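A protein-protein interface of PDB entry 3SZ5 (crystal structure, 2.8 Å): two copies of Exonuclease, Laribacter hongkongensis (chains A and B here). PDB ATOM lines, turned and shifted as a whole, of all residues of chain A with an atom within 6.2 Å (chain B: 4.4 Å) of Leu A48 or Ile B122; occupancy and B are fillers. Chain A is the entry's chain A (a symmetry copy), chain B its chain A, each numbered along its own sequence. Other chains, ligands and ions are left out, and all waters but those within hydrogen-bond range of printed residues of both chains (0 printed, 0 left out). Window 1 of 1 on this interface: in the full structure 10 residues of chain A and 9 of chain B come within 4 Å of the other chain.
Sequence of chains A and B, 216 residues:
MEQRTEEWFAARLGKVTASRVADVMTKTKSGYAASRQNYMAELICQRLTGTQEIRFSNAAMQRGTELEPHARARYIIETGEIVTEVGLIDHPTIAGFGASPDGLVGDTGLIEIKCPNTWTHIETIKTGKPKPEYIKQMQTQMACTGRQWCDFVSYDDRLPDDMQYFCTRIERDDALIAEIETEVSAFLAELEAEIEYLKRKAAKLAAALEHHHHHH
Of the 13 printed residues of chain A, 7 touch a printed residue of chain B.
Printed residues of chain A that touch a printed residue of chain B: Ile A44, Cys A45, Leu A48, Thr A49, Glu A194, Leu A198 and Lys A199.
Hydrophobic or aromatic side chains of chain A within 4 Å of the printed part of chain B: Ile A44, Leu A48 and Leu A198.
Along chain A the printed residues that touch a printed residue of chain B span positions 44 to 199.
Printed residues of chain B that touch a printed residue of chain A: Thr B118, Trp B119, Ile B122, Lys B126, Leu B159, Pro B160 and Met B163.
Along chain B the printed residues that touch a printed residue of chain A span positions 118 to 163.
Among the printed residues, Asp or Glu carboxylates within 4 Å of a Lys or Arg side-chain nitrogen of the other chain: Glu A194 with Lys B126.
Among the printed residues, pairs that only touch across the chains: Ile A44 with Trp B119 (3.97 Å), Cys A45 with Thr B118 (3.7 Å), Cys A45 with Ile B122 (3.95 Å), Leu A48 with Ile B122 (3.998 Å), Leu A48 with Leu B159 (3.9 Å), Leu A48 with Pro B160 (3.5 Å), Thr A49 with Thr B118 (3.9 Å), Thr A49 with Leu B159 (3.7 Å), Leu A198 with Lys B126 (3.99 Å), Leu A198 with Met B163 (3.6 Å) and Lys A199 with Met B163 (3.7 Å).
The side-chain carboxylate of Glu A194 is in salt-bridge range of the side-chain amino group of Lys B126 (3.5 Å).
SG of Cys A45 sits at hydrogen-bond distance from N of Trp B119.
No position is printed for both chains.
Of the 13 pairs that touch across the chains among the printed residues, none has its exchanged pair printed and touching as well.
O of Cys A45 lies within hydrogen-bond range of OG1 of Thr A49, at 2.7 Å.
The side-chain hydroxyl of Thr A49 is in hydrogen-bond range of the backbone carbonyl oxygen of Thr A51, 3.1 Å away.
NE1 of Trp B119 sits close to OE2 of Glu B123, at 3.3 Å.
Of the printed residues of chain B, Ile A44 touches Trp B119.
Arg A47 touches none of the printed residues of chain B.
Of the printed residues of chain B, Leu A48 touches Ile B122, Leu B159 and Pro B160.
Printed residues of chain B within 4 Å of Glu A194: Lys B126 (3.5 Å).
Of the printed residues of chain B, Lys A199 touches Met B163.
Of the printed residues of chain A, Ile B122 touches Cys A45 (3.95 Å) and Leu A48 (3.998 Å).
Of the printed residues of chain A, Lys B126 touches Glu A194 (3.5 Å) and Leu A198 (3.99 Å).
The nearest printed residue of chain A that does not touch Ile B122 is Leu A198 (4.3 Å).
The nearest printed residue of chain A that does not touch Lys B126 is Ile A44 (6.8 Å).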
ATOM      1  N   LEU A  43     -27.537 -17.033 -29.071  1.00  0.00           N
ATOM      2  CA  LEU A  43     -28.841 -16.990 -28.460  1.00  0.00           C
ATOM      3  C   LEU A  43     -29.094 -18.242 -27.622  1.00  0.00           C
ATOM      4  O   LEU A  43     -29.735 -18.167 -26.563  1.00  0.00           O
ATOM      5  CB  LEU A  43     -29.918 -16.796 -29.514  1.00  0.00           C
ATOM      6  CG  LEU A  43     -29.862 -15.520 -30.368  1.00  0.00           C
ATOM      7  CD1 LEU A  43     -31.025 -15.511 -31.325  1.00  0.00           C
ATOM      8  CD2 LEU A  43     -29.846 -14.224 -29.546  1.00  0.00           C
ATOM      9  N   ILE A  44     -28.557 -19.376 -28.074  1.00  0.00           N
ATOM     10  CA  ILE A  44     -28.620 -20.593 -27.277  1.00  0.00           C
ATOM     11  C   ILE A  44     -27.914 -20.369 -25.951  1.00  0.00           C
ATOM     12  O   ILE A  44     -28.424 -20.770 -24.890  1.00  0.00           O
ATOM     13  CB  ILE A  44     -27.990 -21.798 -27.987  1.00  0.00           C
ATOM     14  CG1 ILE A  44     -28.921 -22.292 -29.108  1.00  0.00           C
ATOM     15  CG2 ILE A  44     -27.695 -22.934 -26.961  1.00  0.00           C
ATOM     16  CD1 ILE A  44     -28.279 -23.213 -30.098  1.00  0.00           C
ATOM     17  N   CYS A  45     -26.752 -19.718 -26.013  1.00  0.00           N
ATOM     18  CA  CYS A  45     -25.970 -19.476 -24.823  1.00  0.00           C
ATOM     19  C   CYS A  45     -26.648 -18.455 -23.938  1.00  0.00           C
ATOM     20  O   CYS A  45     -26.635 -18.597 -22.707  1.00  0.00           O
ATOM     21  CB  CYS A  45     -24.548 -19.079 -25.175  1.00  0.00           C
ATOM     22  SG  CYS A  45     -23.652 -20.498 -25.863  1.00  0.00           S
ATOM     23  N   GLN A  46     -27.269 -17.452 -24.557  1.00  0.00           N
ATOM     24  CA  GLN A  46     -27.991 -16.452 -23.785  1.00  0.00           C
ATOM     25  C   GLN A  46     -29.097 -17.104 -22.982  1.00  0.00           C
ATOM     26  O   GLN A  46     -29.177 -16.930 -21.762  1.00  0.00           O
ATOM     27  CB  GLN A  46     -28.558 -15.359 -24.675  1.00  0.00           C
ATOM     28  CG  GLN A  46     -27.536 -14.294 -24.953  1.00  0.00           C
ATOM     29  CD  GLN A  46     -27.980 -13.261 -25.960  1.00  0.00           C
ATOM     30  OE1 GLN A  46     -29.176 -13.033 -26.160  1.00  0.00           O
ATOM     31  NE2 GLN A  46     -27.016 -12.618 -26.591  1.00  0.00           N
ATOM     32  N   ARG A  47     -29.926 -17.884 -23.661  1.00  0.00           N
ATOM     33  CA  ARG A  47     -31.030 -18.532 -22.994  1.00  0.00           C
ATOM     34  C   ARG A  47     -30.574 -19.473 -21.887  1.00  0.00           C
ATOM     35  O   ARG A  47     -31.190 -19.501 -20.821  1.00  0.00           O
ATOM     36  CB  ARG A  47     -31.907 -19.247 -23.992  1.00  0.00           C
ATOM     37  CG  ARG A  47     -32.710 -18.296 -24.813  1.00  0.00           C
ATOM     38  CD  ARG A  47     -33.589 -19.045 -25.722  1.00  0.00           C
ATOM     39  NE  ARG A  47     -34.254 -18.180 -26.683  1.00  0.00           N
ATOM     40  CZ  ARG A  47     -35.489 -18.394 -27.135  1.00  0.00           C
ATOM     41  NH1 ARG A  47     -36.183 -19.451 -26.697  1.00  0.00           N
ATOM     42  NH2 ARG A  47     -36.034 -17.557 -28.010  1.00  0.00           N
ATOM     43  N   LEU A  48     -29.488 -20.213 -22.119  1.00  0.00           N
ATOM     44  CA  LEU A  48     -29.009 -21.182 -21.136  1.00  0.00           C
ATOM     45  C   LEU A  48     -28.293 -20.550 -19.964  1.00  0.00           C
ATOM     46  O   LEU A  48     -28.514 -20.936 -18.821  1.00  0.00           O
ATOM     47  CB  LEU A  48     -28.103 -22.212 -21.790  1.00  0.00           C
ATOM     48  CG  LEU A  48     -28.774 -23.297 -22.635  1.00  0.00           C
ATOM     49  CD1 LEU A  48     -27.723 -24.075 -23.408  1.00  0.00           C
ATOM     50  CD2 LEU A  48     -29.642 -24.239 -21.797  1.00  0.00           C
ATOM     51  N   THR A  49     -27.435 -19.578 -20.241  1.00  0.00           N
ATOM     52  CA  THR A  49     -26.617 -18.990 -19.184  1.00  0.00           C
ATOM     53  C   THR A  49     -27.325 -17.854 -18.449  1.00  0.00           C
ATOM     54  O   THR A  49     -26.962 -17.533 -17.324  1.00  0.00           O
ATOM     55  CB  THR A  49     -25.273 -18.462 -19.708  1.00  0.00           C
ATOM     56  OG1 THR A  49     -25.518 -17.335 -20.556  1.00  0.00           O
ATOM     57  CG2 THR A  49     -24.496 -19.544 -20.466  1.00  0.00           C
ATOM     58  N   GLY A  50     -28.317 -17.238 -19.082  1.00  0.00           N
ATOM     59  CA  GLY A  50     -29.012 -16.124 -18.479  1.00  0.00           C
ATOM     60  C   GLY A  50     -28.285 -14.789 -18.539  1.00  0.00           C
ATOM     61  O   GLY A  50     -28.652 -13.871 -17.805  1.00  0.00           O
ATOM     62  N   THR A  51     -27.245 -14.675 -19.380  1.00  0.00           N
ATOM     63  CA  THR A  51     -26.667 -13.370 -19.783  1.00  0.00           C
ATOM     64  C   THR A  51     -25.912 -13.406 -21.104  1.00  0.00           C
ATOM     65  O   THR A  51     -25.761 -14.465 -21.728  1.00  0.00           O
ATOM     66  CB  THR A  51     -25.663 -12.783 -18.779  1.00  0.00           C
ATOM     67  OG1 THR A  51     -25.001 -13.854 -18.106  1.00  0.00           O
ATOM     68  CG2 THR A  51     -26.340 -11.765 -17.796  1.00  0.00           C
ATOM     69  N   GLU A 194     -33.133 -27.148 -30.133  1.00  0.00           N
ATOM     70  CA  GLU A 194     -31.760 -27.365 -29.722  1.00  0.00           C
ATOM     71  C   GLU A 194     -31.557 -27.244 -28.196  1.00  0.00           C
ATOM     72  O   GLU A 194     -30.835 -28.038 -27.600  1.00  0.00           O
ATOM     73  CB  GLU A 194     -30.855 -26.403 -30.491  1.00  0.00           C
ATOM     74  CG  GLU A 194     -29.411 -26.561 -30.197  1.00  0.00           C
ATOM     75  CD  GLU A 194     -28.663 -27.333 -31.246  1.00  0.00           C
ATOM     76  OE1 GLU A 194     -29.041 -27.236 -32.442  1.00  0.00           O
ATOM     77  OE2 GLU A 194     -27.670 -28.013 -30.860  1.00  0.00           O
ATOM     78  N   ILE A 195     -32.202 -26.263 -27.573  1.00  0.00           N
ATOM     79  CA  ILE A 195     -32.135 -26.061 -26.131  1.00  0.00           C
ATOM     80  C   ILE A 195     -32.800 -27.230 -25.394  1.00  0.00           C
ATOM     81  O   ILE A 195     -32.251 -27.818 -24.475  1.00  0.00           O
ATOM     82  CB  ILE A 195     -32.804 -24.717 -25.787  1.00  0.00           C
ATOM     83  CG1 ILE A 195     -31.848 -23.585 -26.165  1.00  0.00           C
ATOM     84  CG2 ILE A 195     -33.265 -24.660 -24.300  1.00  0.00           C
ATOM     85  CD1 ILE A 195     -32.327 -22.221 -25.829  1.00  0.00           C
ATOM     86  N   LEU A 198     -30.752 -30.389 -25.744  1.00  0.00           N
ATOM     87  CA  LEU A 198     -29.679 -30.342 -24.762  1.00  0.00           C
ATOM     88  C   LEU A 198     -30.155 -30.576 -23.321  1.00  0.00           C
ATOM     89  O   LEU A 198     -29.532 -31.324 -22.561  1.00  0.00           O
ATOM     90  CB  LEU A 198     -28.955 -29.014 -24.876  1.00  0.00           C
ATOM     91  CG  LEU A 198     -27.774 -28.967 -25.835  1.00  0.00           C
ATOM     92  CD1 LEU A 198     -27.575 -30.257 -26.645  1.00  0.00           C
ATOM     93  CD2 LEU A 198     -27.902 -27.742 -26.748  1.00  0.00           C
ATOM     94  N   LYS A 199     -31.268 -29.942 -22.958  1.00  0.00           N
ATOM     95  CA  LYS A 199     -31.816 -30.080 -21.618  1.00  0.00           C
ATOM     96  C   LYS A 199     -32.159 -31.528 -21.340  1.00  0.00           C
ATOM     97  O   LYS A 199     -31.958 -32.022 -20.220  1.00  0.00           O
ATOM     98  CB  LYS A 199     -33.042 -29.190 -21.422  1.00  0.00           C
ATOM     99  CG  LYS A 199     -32.699 -27.744 -21.114  1.00  0.00           C
ATOM    100  CD  LYS A 199     -33.921 -26.997 -20.628  1.00  0.00           C
ATOM    101  CE  LYS A 199     -33.695 -25.487 -20.611  1.00  0.00           C
ATOM    102  NZ  LYS A 199     -34.926 -24.744 -20.215  1.00  0.00           N
ATOM    103  N   THR B 118     -18.647 -20.914 -23.503  1.00  0.00           N
ATOM    104  CA  THR B 118     -19.841 -21.720 -23.383  1.00  0.00           C
ATOM    105  C   THR B 118     -20.169 -22.548 -24.632  1.00  0.00           C
ATOM    106  O   THR B 118     -20.357 -23.775 -24.538  1.00  0.00           O
ATOM    107  CB  THR B 118     -21.035 -20.867 -23.032  1.00  0.00           C
ATOM    108  OG1 THR B 118     -20.727 -20.066 -21.879  1.00  0.00           O
ATOM    109  CG2 THR B 118     -22.195 -21.749 -22.711  1.00  0.00           C
ATOM    110  N   TRP B 119     -20.225 -21.912 -25.802  1.00  0.00           N
ATOM    111  CA  TRP B 119     -20.653 -22.659 -26.974  1.00  0.00           C
ATOM    112  C   TRP B 119     -19.711 -23.810 -27.298  1.00  0.00           C
ATOM    113  O   TRP B 119     -20.140 -24.877 -27.747  1.00  0.00           O
ATOM    114  CB  TRP B 119     -20.830 -21.775 -28.186  1.00  0.00           C
ATOM    115  CG  TRP B 119     -21.239 -22.612 -29.363  1.00  0.00           C
ATOM    116  CD1 TRP B 119     -20.512 -22.841 -30.491  1.00  0.00           C
ATOM    117  CD2 TRP B 119     -22.450 -23.391 -29.500  1.00  0.00           C
ATOM    118  NE1 TRP B 119     -21.197 -23.684 -31.338  1.00  0.00           N
ATOM    119  CE2 TRP B 119     -22.392 -24.030 -30.761  1.00  0.00           C
ATOM    120  CE3 TRP B 119     -23.586 -23.589 -28.688  1.00  0.00           C
ATOM    121  CZ2 TRP B 119     -23.418 -24.861 -31.233  1.00  0.00           C
ATOM    122  CZ3 TRP B 119     -24.616 -24.407 -29.157  1.00  0.00           C
ATOM    123  CH2 TRP B 119     -24.520 -25.038 -30.417  1.00  0.00           C
ATOM    124  N   THR B 120     -18.422 -23.576 -27.063  1.00  0.00           N
ATOM    125  CA  THR B 120     -17.402 -24.593 -27.233  1.00  0.00           C
ATOM    126  C   THR B 120     -17.642 -25.741 -26.273  1.00  0.00           C
ATOM    127  O   THR B 120     -17.728 -26.894 -26.683  1.00  0.00           O
ATOM    128  CB  THR B 120     -16.033 -24.018 -26.982  1.00  0.00           C
ATOM    129  OG1 THR B 120     -15.826 -22.925 -27.891  1.00  0.00           O
ATOM    130  CG2 THR B 120     -14.974 -25.085 -27.189  1.00  0.00           C
ATOM    131  N   HIS B 121     -17.777 -25.407 -24.997  1.00  0.00           N
ATOM    132  CA  HIS B 121     -18.186 -26.369 -23.986  1.00  0.00           C
ATOM    133  C   HIS B 121     -19.424 -27.194 -24.402  1.00  0.00           C
ATOM    134  O   HIS B 121     -19.414 -28.433 -24.309  1.00  0.00           O
ATOM    135  CB  HIS B 121     -18.419 -25.630 -22.681  1.00  0.00           C
ATOM    136  CG  HIS B 121     -18.670 -26.528 -21.513  1.00  0.00           C
ATOM    137  ND1 HIS B 121     -19.940 -26.833 -21.070  1.00  0.00           N
ATOM    138  CD2 HIS B 121     -17.815 -27.168 -20.681  1.00  0.00           C
ATOM    139  CE1 HIS B 121     -19.852 -27.624 -20.015  1.00  0.00           C
ATOM    140  NE2 HIS B 121     -18.574 -27.849 -19.763  1.00  0.00           N
ATOM    141  N   ILE B 122     -20.463 -26.519 -24.892  1.00  0.00           N
ATOM    142  CA  ILE B 122     -21.637 -27.209 -25.396  1.00  0.00           C
ATOM    143  C   ILE B 122     -21.295 -28.194 -26.512  1.00  0.00           C
ATOM    144  O   ILE B 122     -21.801 -29.327 -26.508  1.00  0.00           O
ATOM    145  CB  ILE B 122     -22.729 -26.242 -25.862  1.00  0.00           C
ATOM    146  CG1 ILE B 122     -23.486 -25.714 -24.645  1.00  0.00           C
ATOM    147  CG2 ILE B 122     -23.707 -26.946 -26.789  1.00  0.00           C
ATOM    148  CD1 ILE B 122     -23.965 -24.281 -24.758  1.00  0.00           C
ATOM    149  N   GLU B 123     -20.428 -27.800 -27.448  1.00  0.00           N
ATOM    150  CA  GLU B 123     -20.093 -28.706 -28.546  1.00  0.00           C
ATOM    151  C   GLU B 123     -19.307 -29.919 -28.053  1.00  0.00           C
ATOM    152  O   GLU B 123     -19.355 -30.990 -28.649  1.00  0.00           O
ATOM    153  CB  GLU B 123     -19.348 -27.989 -29.676  1.00  0.00           C
ATOM    154  CG  GLU B 123     -20.168 -26.886 -30.358  1.00  0.00           C
ATOM    155  CD  GLU B 123     -19.632 -26.482 -31.762  1.00  0.00           C
ATOM    156  OE1 GLU B 123     -18.431 -26.095 -31.883  1.00  0.00           O
ATOM    157  OE2 GLU B 123     -20.436 -26.547 -32.738  1.00  0.00           O
ATOM    158  N   THR B 124     -18.579 -29.748 -26.961  1.00  0.00           N
ATOM    159  CA  THR B 124     -17.816 -30.847 -26.407  1.00  0.00           C
ATOM    160  C   THR B 124     -18.787 -31.852 -25.804  1.00  0.00           C
ATOM    161  O   THR B 124     -18.666 -33.073 -26.027  1.00  0.00           O
ATOM    162  CB  THR B 124     -16.858 -30.359 -25.356  1.00  0.00           C
ATOM    163  OG1 THR B 124     -15.920 -29.485 -25.971  1.00  0.00           O
ATOM    164  CG2 THR B 124     -16.120 -31.511 -24.765  1.00  0.00           C
ATOM    165  N   ILE B 125     -19.758 -31.327 -25.053  1.00  0.00           N
ATOM    166  CA  ILE B 125     -20.844 -32.148 -24.547  1.00  0.00           C
ATOM    167  C   ILE B 125     -21.598 -32.796 -25.711  1.00  0.00           C
ATOM    168  O   ILE B 125     -21.863 -33.992 -25.683  1.00  0.00           O
ATOM    169  CB  ILE B 125     -21.839 -31.332 -23.671  1.00  0.00           C
ATOM    170  CG1 ILE B 125     -21.192 -30.903 -22.341  1.00  0.00           C
ATOM    171  CG2 ILE B 125     -23.092 -32.144 -23.412  1.00  0.00           C
ATOM    172  CD1 ILE B 125     -22.021 -29.942 -21.528  1.00  0.00           C
ATOM    173  N   LYS B 126     -21.939 -32.012 -26.731  1.00  0.00           N
ATOM    174  CA  LYS B 126     -22.711 -32.536 -27.854  1.00  0.00           C
ATOM    175  C   LYS B 126     -22.035 -33.754 -28.484  1.00  0.00           C
ATOM    176  O   LYS B 126     -22.711 -34.705 -28.860  1.00  0.00           O
ATOM    177  CB  LYS B 126     -22.963 -31.463 -28.926  1.00  0.00           C
ATOM    178  CG  LYS B 126     -24.124 -30.502 -28.637  1.00  0.00           C
ATOM    179  CD  LYS B 126     -24.754 -29.939 -29.921  1.00  0.00           C
ATOM    180  CE  LYS B 126     -23.760 -29.108 -30.736  1.00  0.00           C
ATOM    181  NZ  LYS B 126     -24.385 -28.507 -31.964  1.00  0.00           N
ATOM    182  N   LEU B 159     -23.478 -21.969 -17.072  1.00  0.00           N
ATOM    183  CA  LEU B 159     -24.595 -22.828 -17.492  1.00  0.00           C
ATOM    184  C   LEU B 159     -25.338 -23.453 -16.321  1.00  0.00           C
ATOM    185  O   LEU B 159     -24.866 -23.372 -15.191  1.00  0.00           O
ATOM    186  CB  LEU B 159     -24.033 -23.975 -18.311  1.00  0.00           C
ATOM    187  CG  LEU B 159     -23.448 -23.621 -19.660  1.00  0.00           C
ATOM    188  CD1 LEU B 159     -22.625 -24.788 -20.146  1.00  0.00           C
ATOM    189  CD2 LEU B 159     -24.600 -23.290 -20.589  1.00  0.00           C
ATOM    190  N   PRO B 160     -26.490 -24.104 -16.583  1.00  0.00           N
ATOM    191  CA  PRO B 160     -27.171 -24.881 -15.540  1.00  0.00           C
ATOM    192  C   PRO B 160     -26.291 -26.016 -14.989  1.00  0.00           C
ATOM    193  O   PRO B 160     -25.453 -26.575 -15.728  1.00  0.00           O
ATOM    194  CB  PRO B 160     -28.382 -25.452 -16.271  1.00  0.00           C
ATOM    195  CG  PRO B 160     -28.617 -24.530 -17.362  1.00  0.00           C
ATOM    196  CD  PRO B 160     -27.286 -24.070 -17.820  1.00  0.00           C
ATOM    197  N   MET B 163     -25.200 -29.098 -16.742  1.00  0.00           N
ATOM    198  CA  MET B 163     -24.359 -28.874 -17.941  1.00  0.00           C
ATOM    199  C   MET B 163     -22.971 -28.269 -17.696  1.00  0.00           C
ATOM    200  O   MET B 163     -22.238 -28.034 -18.651  1.00  0.00           O
ATOM    201  CB  MET B 163     -25.078 -27.968 -18.922  1.00  0.00           C
ATOM    202  CG  MET B 163     -26.279 -28.610 -19.516  1.00  0.00           C
ATOM    203  SD  MET B 163     -27.060 -27.471 -20.648  1.00  0.00           S
ATOM    204  CE  MET B 163     -28.658 -28.262 -20.974  1.00  0.00           C
